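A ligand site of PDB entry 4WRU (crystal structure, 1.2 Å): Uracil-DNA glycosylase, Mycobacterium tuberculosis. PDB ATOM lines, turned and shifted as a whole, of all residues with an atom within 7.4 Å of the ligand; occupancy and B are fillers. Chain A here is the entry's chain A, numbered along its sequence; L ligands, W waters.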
ATOM      1  N   VAL A  76      17.486  -5.933   9.821  1.00  0.00           N
ATOM      2  CA  VAL A  76      17.710  -6.001   8.353  1.00  0.00           C
ATOM      3  C   VAL A  76      16.719  -5.057   7.710  1.00  0.00           C
ATOM      4  O   VAL A  76      15.522  -5.272   7.748  1.00  0.00           O
ATOM      5  CB  VAL A  76      17.578  -7.373   7.772  1.00  0.00           C
ATOM      6  CG1 VAL A  76      17.990  -7.282   6.320  1.00  0.00           C
ATOM      7  CG2 VAL A  76      18.385  -8.351   8.591  1.00  0.00           C
ATOM      8  N   GLY A  77      17.283  -4.007   7.090  1.00  0.00           N
ATOM      9  CA  GLY A  77      16.521  -3.145   6.213  1.00  0.00           C
ATOM     10  C   GLY A  77      16.713  -3.471   4.738  1.00  0.00           C
ATOM     11  O   GLY A  77      17.228  -4.546   4.375  1.00  0.00           O
ATOM     12  N   GLN A  78      16.312  -2.529   3.898  1.00  0.00           N
ATOM     13  CA  GLN A  78      16.317  -2.723   2.470  1.00  0.00           C
ATOM     14  C   GLN A  78      17.549  -2.218   1.799  1.00  0.00           C
ATOM     15  O   GLN A  78      18.301  -2.983   1.208  1.00  0.00           O
ATOM     16  CB  GLN A  78      15.054  -2.039   1.950  1.00  0.00           C
ATOM     17  CG  GLN A  78      13.783  -2.738   2.434  1.00  0.00           C
ATOM     18  CD  GLN A  78      12.496  -2.049   2.051  1.00  0.00           C
ATOM     19  OE1 GLN A  78      12.483  -1.006   1.376  1.00  0.00           O
ATOM     20  NE2 GLN A  78      11.392  -2.609   2.472  1.00  0.00           N
ATOM     21  N   ASP A  79      17.750  -0.886   1.822  1.00  0.00           N
ATOM     22  CA  ASP A  79      18.898  -0.293   1.224  1.00  0.00           C
ATOM     23  C   ASP A  79      19.148   1.054   1.869  1.00  0.00           C
ATOM     24  O   ASP A  79      18.326   1.550   2.701  1.00  0.00           O
ATOM     25  CB  ASP A  79      18.802  -0.173  -0.308  1.00  0.00           C
ATOM     26  CG  ASP A  79      17.780   0.767  -0.833  1.00  0.00           C
ATOM     27  OD1 ASP A  79      16.775   1.109  -0.178  1.00  0.00           O
ATOM     28  OD2 ASP A  79      18.048   1.256  -2.001  1.00  0.00           O
ATOM     29  N   PRO A  80      20.315   1.646   1.615  1.00  0.00           N
ATOM     30  CA  PRO A  80      20.646   2.861   2.391  1.00  0.00           C
ATOM     31  C   PRO A  80      19.839   4.085   2.104  1.00  0.00           C
ATOM     32  O   PRO A  80      19.178   4.186   1.100  1.00  0.00           O
ATOM     33  CB  PRO A  80      22.142   3.130   2.050  1.00  0.00           C
ATOM     34  CG  PRO A  80      22.621   1.833   1.574  1.00  0.00           C
ATOM     35  CD  PRO A  80      21.476   1.152   0.893  1.00  0.00           C
ATOM     36  N   TYR A  81      19.858   4.985   3.081  1.00  0.00           N
ATOM     37  CA  TYR A  81      19.231   6.299   2.802  1.00  0.00           C
ATOM     38  C   TYR A  81      19.662   6.884   1.477  1.00  0.00           C
ATOM     39  O   TYR A  81      20.854   6.953   1.219  1.00  0.00           O
ATOM     40  CB  TYR A  81      19.464   7.310   3.902  1.00  0.00           C
ATOM     41  CG  TYR A  81      18.885   7.025   5.258  1.00  0.00           C
ATOM     42  CD1 TYR A  81      17.512   6.994   5.423  1.00  0.00           C
ATOM     43  CD2 TYR A  81      19.726   6.825   6.335  1.00  0.00           C
ATOM     44  CE1 TYR A  81      16.964   6.754   6.650  1.00  0.00           C
ATOM     45  CE2 TYR A  81      19.254   6.581   7.598  1.00  0.00           C
ATOM     46  CZ  TYR A  81      17.828   6.513   7.740  1.00  0.00           C
ATOM     47  OH  TYR A  81      17.240   6.296   8.971  1.00  0.00           O
ATOM     48  N   PRO A  82      18.731   7.379   0.676  1.00  0.00           N
ATOM     49  CA  PRO A  82      19.092   7.908  -0.654  1.00  0.00           C
ATOM     50  C   PRO A  82      19.475   9.397  -0.689  1.00  0.00           C
ATOM     51  O   PRO A  82      19.931   9.898  -1.756  1.00  0.00           O
ATOM     52  CB  PRO A  82      17.796   7.653  -1.454  1.00  0.00           C
ATOM     53  CG  PRO A  82      16.759   7.918  -0.434  1.00  0.00           C
ATOM     54  CD  PRO A  82      17.287   7.160   0.773  1.00  0.00           C
ATOM     55  N   ALA A  87      23.206   8.369   4.807  1.00  0.00           N
ATOM     56  CA  ALA A  87      23.684   7.033   5.035  1.00  0.00           C
ATOM     57  C   ALA A  87      25.121   7.000   5.550  1.00  0.00           C
ATOM     58  O   ALA A  87      25.992   7.755   5.096  1.00  0.00           O
ATOM     59  CB  ALA A  87      23.650   6.235   3.764  1.00  0.00           C
ATOM     60  N   VAL A  88      25.348   6.184   6.560  1.00  0.00           N
ATOM     61  CA  VAL A  88      26.694   6.019   7.173  1.00  0.00           C
ATOM     62  C   VAL A  88      27.168   4.609   7.232  1.00  0.00           C
ATOM     63  O   VAL A  88      28.223   4.301   7.837  1.00  0.00           O
ATOM     64  CB  VAL A  88      26.698   6.673   8.595  1.00  0.00           C
ATOM     65  CG1 VAL A  88      26.297   8.149   8.519  1.00  0.00           C
ATOM     66  CG2 VAL A  88      25.786   5.897   9.576  1.00  0.00           C
ATOM     67  N   GLY A  89      26.441   3.672   6.601  1.00  0.00           N
ATOM     68  CA  GLY A  89      26.924   2.279   6.593  1.00  0.00           C
ATOM     69  C   GLY A  89      26.445   1.401   7.757  1.00  0.00           C
ATOM     70  O   GLY A  89      26.692   0.193   7.738  1.00  0.00           O
ATOM     71  N   LEU A  90      25.795   1.992   8.748  1.00  0.00           N
ATOM     72  CA  LEU A  90      25.020   1.247   9.721  1.00  0.00           C
ATOM     73  C   LEU A  90      23.559   1.536   9.320  1.00  0.00           C
ATOM     74  O   LEU A  90      23.137   2.683   9.254  1.00  0.00           O
ATOM     75  CB  LEU A  90      25.365   1.738  11.083  1.00  0.00           C
ATOM     76  CG  LEU A  90      26.759   1.568  11.626  1.00  0.00           C
ATOM     77  CD1 LEU A  90      26.901   2.142  13.029  1.00  0.00           C
ATOM     78  CD2 LEU A  90      27.215   0.115  11.585  1.00  0.00           C
ATOM     79  N   SER A  91      22.784   0.493   9.048  1.00  0.00           N
ATOM     80  CA  SER A  91      21.394   0.716   8.621  1.00  0.00           C
ATOM     81  C   SER A  91      20.641   1.635   9.616  1.00  0.00           C
ATOM     82  O   SER A  91      20.815   1.509  10.811  1.00  0.00           O
ATOM     83  CB  SER A  91      20.687  -0.552   8.315  1.00  0.00           C
ATOM     84  OG  SER A  91      20.454  -1.336   9.461  1.00  0.00           O
ATOM     85  N   PHE A  92      19.935   2.623   9.038  1.00  0.00           N
ATOM     86  CA  PHE A  92      19.027   3.542   9.728  1.00  0.00           C
ATOM     87  C   PHE A  92      19.752   4.623  10.498  1.00  0.00           C
ATOM     88  O   PHE A  92      19.075   5.644  10.751  1.00  0.00           O
ATOM     89  CB  PHE A  92      17.985   2.799  10.555  1.00  0.00           C
ATOM     90  CG  PHE A  92      17.168   1.862   9.711  1.00  0.00           C
ATOM     91  CD1 PHE A  92      16.120   2.335   8.975  1.00  0.00           C
ATOM     92  CD2 PHE A  92      17.458   0.479   9.668  1.00  0.00           C
ATOM     93  CE1 PHE A  92      15.391   1.523   8.141  1.00  0.00           C
ATOM     94  CE2 PHE A  92      16.689  -0.329   8.870  1.00  0.00           C
ATOM     95  CZ  PHE A  92      15.683   0.181   8.097  1.00  0.00           C
ATOM     96  N   SER A  93      21.047   4.530  10.757  1.00  0.00           N
ATOM     97  CA  SER A  93      21.767   5.472  11.540  1.00  0.00           C
ATOM     98  C   SER A  93      22.110   6.739  10.712  1.00  0.00           C
ATOM     99  O   SER A  93      22.216   6.705   9.468  1.00  0.00           O
ATOM    100  CB  SER A  93      23.091   4.813  12.016  1.00  0.00           C
ATOM    101  OG  SER A  93      23.705   5.567  13.042  1.00  0.00           O
ATOM    102  N   PRO A 102      15.988  11.405   9.321  1.00  0.00           N
ATOM    103  CA  PRO A 102      15.231  10.858   8.240  1.00  0.00           C
ATOM    104  C   PRO A 102      13.935  10.193   8.797  1.00  0.00           C
ATOM    105  O   PRO A 102      13.899   9.728   9.953  1.00  0.00           O
ATOM    106  CB  PRO A 102      16.124   9.754   7.695  1.00  0.00           C
ATOM    107  CG  PRO A 102      17.494  10.094   8.157  1.00  0.00           C
ATOM    108  CD  PRO A 102      17.376  10.910   9.388  1.00  0.00           C
ATOM    109  N   SER A 104      12.390   7.330   8.417  1.00  0.00           N
ATOM    110  CA  SER A 104      12.412   5.982   8.973  1.00  0.00           C
ATOM    111  C   SER A 104      12.939   6.022  10.398  1.00  0.00           C
ATOM    112  O   SER A 104      12.463   5.295  11.250  1.00  0.00           O
ATOM    113  CB  SER A 104      13.306   5.002   8.202  1.00  0.00           C
ATOM    114  OG  SER A 104      12.776   4.566   6.962  1.00  0.00           O
ATOM    115  N   LEU A 105      13.961   6.838  10.634  1.00  0.00           N
ATOM    116  CA  LEU A 105      14.617   6.867  11.948  1.00  0.00           C
ATOM    117  C   LEU A 105      13.621   7.540  12.939  1.00  0.00           C
ATOM    118  O   LEU A 105      13.529   7.129  14.105  1.00  0.00           O
ATOM    119  CB  LEU A 105      15.937   7.576  11.882  1.00  0.00           C
ATOM    120  CG  LEU A 105      16.753   7.584  13.170  1.00  0.00           C
ATOM    121  CD1 LEU A 105      17.050   6.176  13.646  1.00  0.00           C
ATOM    122  CD2 LEU A 105      18.028   8.360  12.939  1.00  0.00           C
ATOM    123  N   ILE A 108      11.294   4.874  13.847  1.00  0.00           N
ATOM    124  CA  ILE A 108      11.990   3.946  14.759  1.00  0.00           C
ATOM    125  C   ILE A 108      12.004   4.459  16.178  1.00  0.00           C
ATOM    126  O   ILE A 108      11.715   3.733  17.132  1.00  0.00           O
ATOM    127  CB  ILE A 108      13.435   3.609  14.197  1.00  0.00           C
ATOM    128  CG1 ILE A 108      13.275   2.720  12.951  1.00  0.00           C
ATOM    129  CG2 ILE A 108      14.238   2.929  15.206  1.00  0.00           C
ATOM    130  CD1 ILE A 108      14.552   2.688  12.161  1.00  0.00           C
ATOM    131  N   LEU A 136      23.481  -3.725  12.211  1.00  0.00           N
ATOM    132  CA  LEU A 136      22.576  -2.840  11.461  1.00  0.00           C
ATOM    133  C   LEU A 136      22.810  -2.999   9.980  1.00  0.00           C
ATOM    134  O   LEU A 136      23.591  -2.314   9.357  1.00  0.00           O
ATOM    135  CB  LEU A 136      22.724  -1.412  11.930  1.00  0.00           C
ATOM    136  CG  LEU A 136      22.484  -1.192  13.412  1.00  0.00           C
ATOM    137  CD1 LEU A 136      23.016   0.133  13.900  1.00  0.00           C
ATOM    138  CD2 LEU A 136      21.028  -1.276  13.651  1.00  0.00           C
ATOM    139  N   LEU A 137      22.159  -4.027   9.460  1.00  0.00           N
ATOM    140  CA  LEU A 137      22.326  -4.499   8.091  1.00  0.00           C
ATOM    141  C   LEU A 137      21.274  -3.941   7.153  1.00  0.00           C
ATOM    142  O   LEU A 137      20.106  -3.656   7.581  1.00  0.00           O
ATOM    143  CB  LEU A 137      22.238  -6.038   8.070  1.00  0.00           C
ATOM    144  CG  LEU A 137      22.700  -6.756   6.797  1.00  0.00           C
ATOM    145  CD1 LEU A 137      24.088  -6.381   6.432  1.00  0.00           C
ATOM    146  CD2 LEU A 137      22.636  -8.270   6.981  1.00  0.00           C
ATOM    147  N   ASN A 138      21.642  -3.822   5.866  1.00  0.00           N
ATOM    148  CA  ASN A 138      20.700  -3.656   4.783  1.00  0.00           C
ATOM    149  C   ASN A 138      20.915  -4.830   3.828  1.00  0.00           C
ATOM    150  O   ASN A 138      21.988  -5.301   3.703  1.00  0.00           O
ATOM    151  CB  ASN A 138      20.879  -2.335   4.079  1.00  0.00           C
ATOM    152  CG  ASN A 138      20.239  -1.182   4.754  1.00  0.00           C
ATOM    153  OD1 ASN A 138      19.083  -1.247   5.224  1.00  0.00           O
ATOM    154  ND2 ASN A 138      21.005  -0.103   4.880  1.00  0.00           N
ATOM    155  N   ARG A 139      19.841  -5.255   3.172  1.00  0.00           N
ATOM    156  CA  ARG A 139      19.946  -6.284   2.150  1.00  0.00           C
ATOM    157  C   ARG A 139      20.854  -5.873   1.023  1.00  0.00           C
ATOM    158  O   ARG A 139      21.551  -6.714   0.474  1.00  0.00           O
ATOM    159  CB  ARG A 139      18.574  -6.686   1.635  1.00  0.00           C
ATOM    160  CG  ARG A 139      18.426  -7.865   0.770  1.00  0.00           C
ATOM    161  CD  ARG A 139      18.453  -9.177   1.537  1.00  0.00           C
ATOM    162  NE  ARG A 139      18.173 -10.182   0.539  1.00  0.00           N
ATOM    163  CZ  ARG A 139      19.058 -11.072   0.102  1.00  0.00           C
ATOM    164  NH1 ARG A 139      20.302 -11.143   0.625  1.00  0.00           N
ATOM    165  NH2 ARG A 139      18.677 -11.958  -0.816  1.00  0.00           N
ATOM    166  N   VAL A 140      20.827  -4.599   0.640  1.00  0.00           N
ATOM    167  CA  VAL A 140      21.645  -4.011  -0.443  1.00  0.00           C
ATOM    168  C   VAL A 140      22.412  -2.875   0.225  1.00  0.00           C
ATOM    169  O   VAL A 140      21.837  -2.086   0.975  1.00  0.00           O
ATOM    170  CB  VAL A 140      20.694  -3.515  -1.589  1.00  0.00           C
ATOM    171  CG1 VAL A 140      21.370  -2.696  -2.643  1.00  0.00           C
ATOM    172  CG2 VAL A 140      19.983  -4.703  -2.213  1.00  0.00           C
ATOM    173  N   TRP A 179      12.661  -5.831   8.646  1.00  0.00           N
ATOM    174  CA  TRP A 179      11.828  -4.665   8.358  1.00  0.00           C
ATOM    175  C   TRP A 179      11.625  -4.557   6.887  1.00  0.00           C
ATOM    176  O   TRP A 179      12.527  -4.174   6.126  1.00  0.00           O
ATOM    177  CB  TRP A 179      12.392  -3.439   8.952  1.00  0.00           C
ATOM    178  CG  TRP A 179      12.303  -3.280  10.422  1.00  0.00           C
ATOM    179  CD1 TRP A 179      11.436  -3.923  11.268  1.00  0.00           C
ATOM    180  CD2 TRP A 179      13.097  -2.442  11.253  1.00  0.00           C
ATOM    181  NE1 TRP A 179      11.646  -3.507  12.541  1.00  0.00           N
ATOM    182  CE2 TRP A 179      12.646  -2.595  12.582  1.00  0.00           C
ATOM    183  CE3 TRP A 179      14.173  -1.553  11.010  1.00  0.00           C
ATOM    184  CZ2 TRP A 179      13.254  -1.959  13.643  1.00  0.00           C
ATOM    185  CZ3 TRP A 179      14.778  -0.947  12.072  1.00  0.00           C
ATOM    186  CH2 TRP A 179      14.261  -1.067  13.361  1.00  0.00           C
ATOM    187  N   HIS A 202       8.060  -1.993   7.170  1.00  0.00           N
ATOM    188  CA  HIS A 202       9.220  -1.149   7.280  1.00  0.00           C
ATOM    189  C   HIS A 202       8.823   0.158   7.917  1.00  0.00           C
ATOM    190  O   HIS A 202       7.724   0.630   7.711  1.00  0.00           O
ATOM    191  CB  HIS A 202       9.793  -1.026   5.853  1.00  0.00           C
ATOM    192  CG  HIS A 202      11.099  -0.349   5.729  1.00  0.00           C
ATOM    193  ND1 HIS A 202      11.278   1.017   5.856  1.00  0.00           N
ATOM    194  CD2 HIS A 202      12.319  -0.852   5.486  1.00  0.00           C
ATOM    195  CE1 HIS A 202      12.539   1.314   5.655  1.00  0.00           C
ATOM    196  NE2 HIS A 202      13.194   0.194   5.422  1.00  0.00           N
ATOM    197  N   PRO A 203       9.780   0.821   8.615  1.00  0.00           N
ATOM    198  CA  PRO A 203       9.511   2.119   9.227  1.00  0.00           C
ATOM    199  C   PRO A 203       9.471   3.315   8.242  1.00  0.00           C
ATOM    200  O   PRO A 203       9.286   4.424   8.739  1.00  0.00           O
ATOM    201  CB  PRO A 203      10.651   2.278  10.202  1.00  0.00           C
ATOM    202  CG  PRO A 203      11.762   1.502   9.660  1.00  0.00           C
ATOM    203  CD  PRO A 203      11.085   0.302   9.044  1.00  0.00           C
ATOM    204  N   SER A 204       9.588   3.128   6.943  1.00  0.00           N
ATOM    205  CA  SER A 204       9.603   4.241   5.981  1.00  0.00           C
ATOM    206  C   SER A 204       8.320   4.962   5.979  1.00  0.00           C
ATOM    207  O   SER A 204       7.344   4.497   6.524  1.00  0.00           O
ATOM    208  CB  SER A 204       9.873   3.702   4.585  1.00  0.00           C
ATOM    209  OG  SER A 204       8.762   3.051   3.987  1.00  0.00           O
HETATM  210  N1  LIG L   1      15.897   2.433   4.751  1.00  0.00           N
HETATM  211  C1  LIG L   1      16.461   1.221   4.925  1.00  0.00           C
HETATM  212  O1  LIG L   1      15.806   0.189   4.598  1.00  0.00           O
HETATM  213  N2  LIG L   1      17.707   1.170   5.478  1.00  0.00           N
HETATM  214  C2  LIG L   1      18.425   2.267   5.760  1.00  0.00           C
HETATM  215  O2  LIG L   1      19.601   2.127   6.170  1.00  0.00           O
HETATM  216  C3  LIG L   1      17.816   3.503   5.603  1.00  0.00           C
HETATM  217  C4  LIG L   1      16.563   3.585   5.084  1.00  0.00           C
HETATM  218  O   HOH W   1      21.485   4.114   5.440  1.00  0.00           O
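A ring nitrogen (ND1) of His 202 sits at hydrogen-bond distance from the backbone NH of Ser 204. The side-chain amide oxygen of Asn 138 is in hydrogen-bond range of the backbone NH of Gln 78. The backbone carbonyl oxygen (O) of Gln 78 sits at hydrogen-bond distance from the backbone NH (N) of Val 140 (3.1 Å). The backbone carbonyl oxygen of Gln 78 sits at hydrogen-bond distance from the backbone NH of Arg 139 (3.4 Å). The side-chain hydroxyl (OH) of Tyr 81 sits at hydrogen-bond distance from the backbone carbonyl oxygen (O) of Phe 92 (2.6 Å). N of Ser 91 lies within hydrogen-bond range of O of Leu 136, at 2.9 Å. The backbone NH of Gly 77 sits at hydrogen-bond distance from the backbone carbonyl oxygen of Leu 137 (2.9 Å). The backbone carbonyl oxygen of Gly 77 sits at hydrogen-bond distance from the backbone NH of Arg 139 (3.0 Å).
CA of Gly 77 touches O1 of the ligand (3.8 Å). Pro 80 touches the ligand (CA to O2, 3.99 Å). Tyr 81 touches the ligand (CD1 to C3, 3.5 Å). Ser 91 touches the ligand (CA to O2, 3.3 Å).
O1 of the ligand sits at hydrogen-bond distance from NE2 of His 202. N2 of the ligand lies within hydrogen-bond range of OD1 of Asn 138 (2.8 Å). The backbone NH (N) of Gln 78 lies within hydrogen-bond range of an oxygen (O1) of the ligand, at 2.9 Å. A nitrogen (N2) of the ligand is in hydrogen-bond range of the backbone carbonyl oxygen (O) of Asp 79, 2.9 Å away. The backbone NH of Phe 92 sits at hydrogen-bond distance from an oxygen (O2) of the ligand.
Water W1 bridges O2 of the ligand (2.8 Å) and N of Tyr 81 (3.0 Å).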
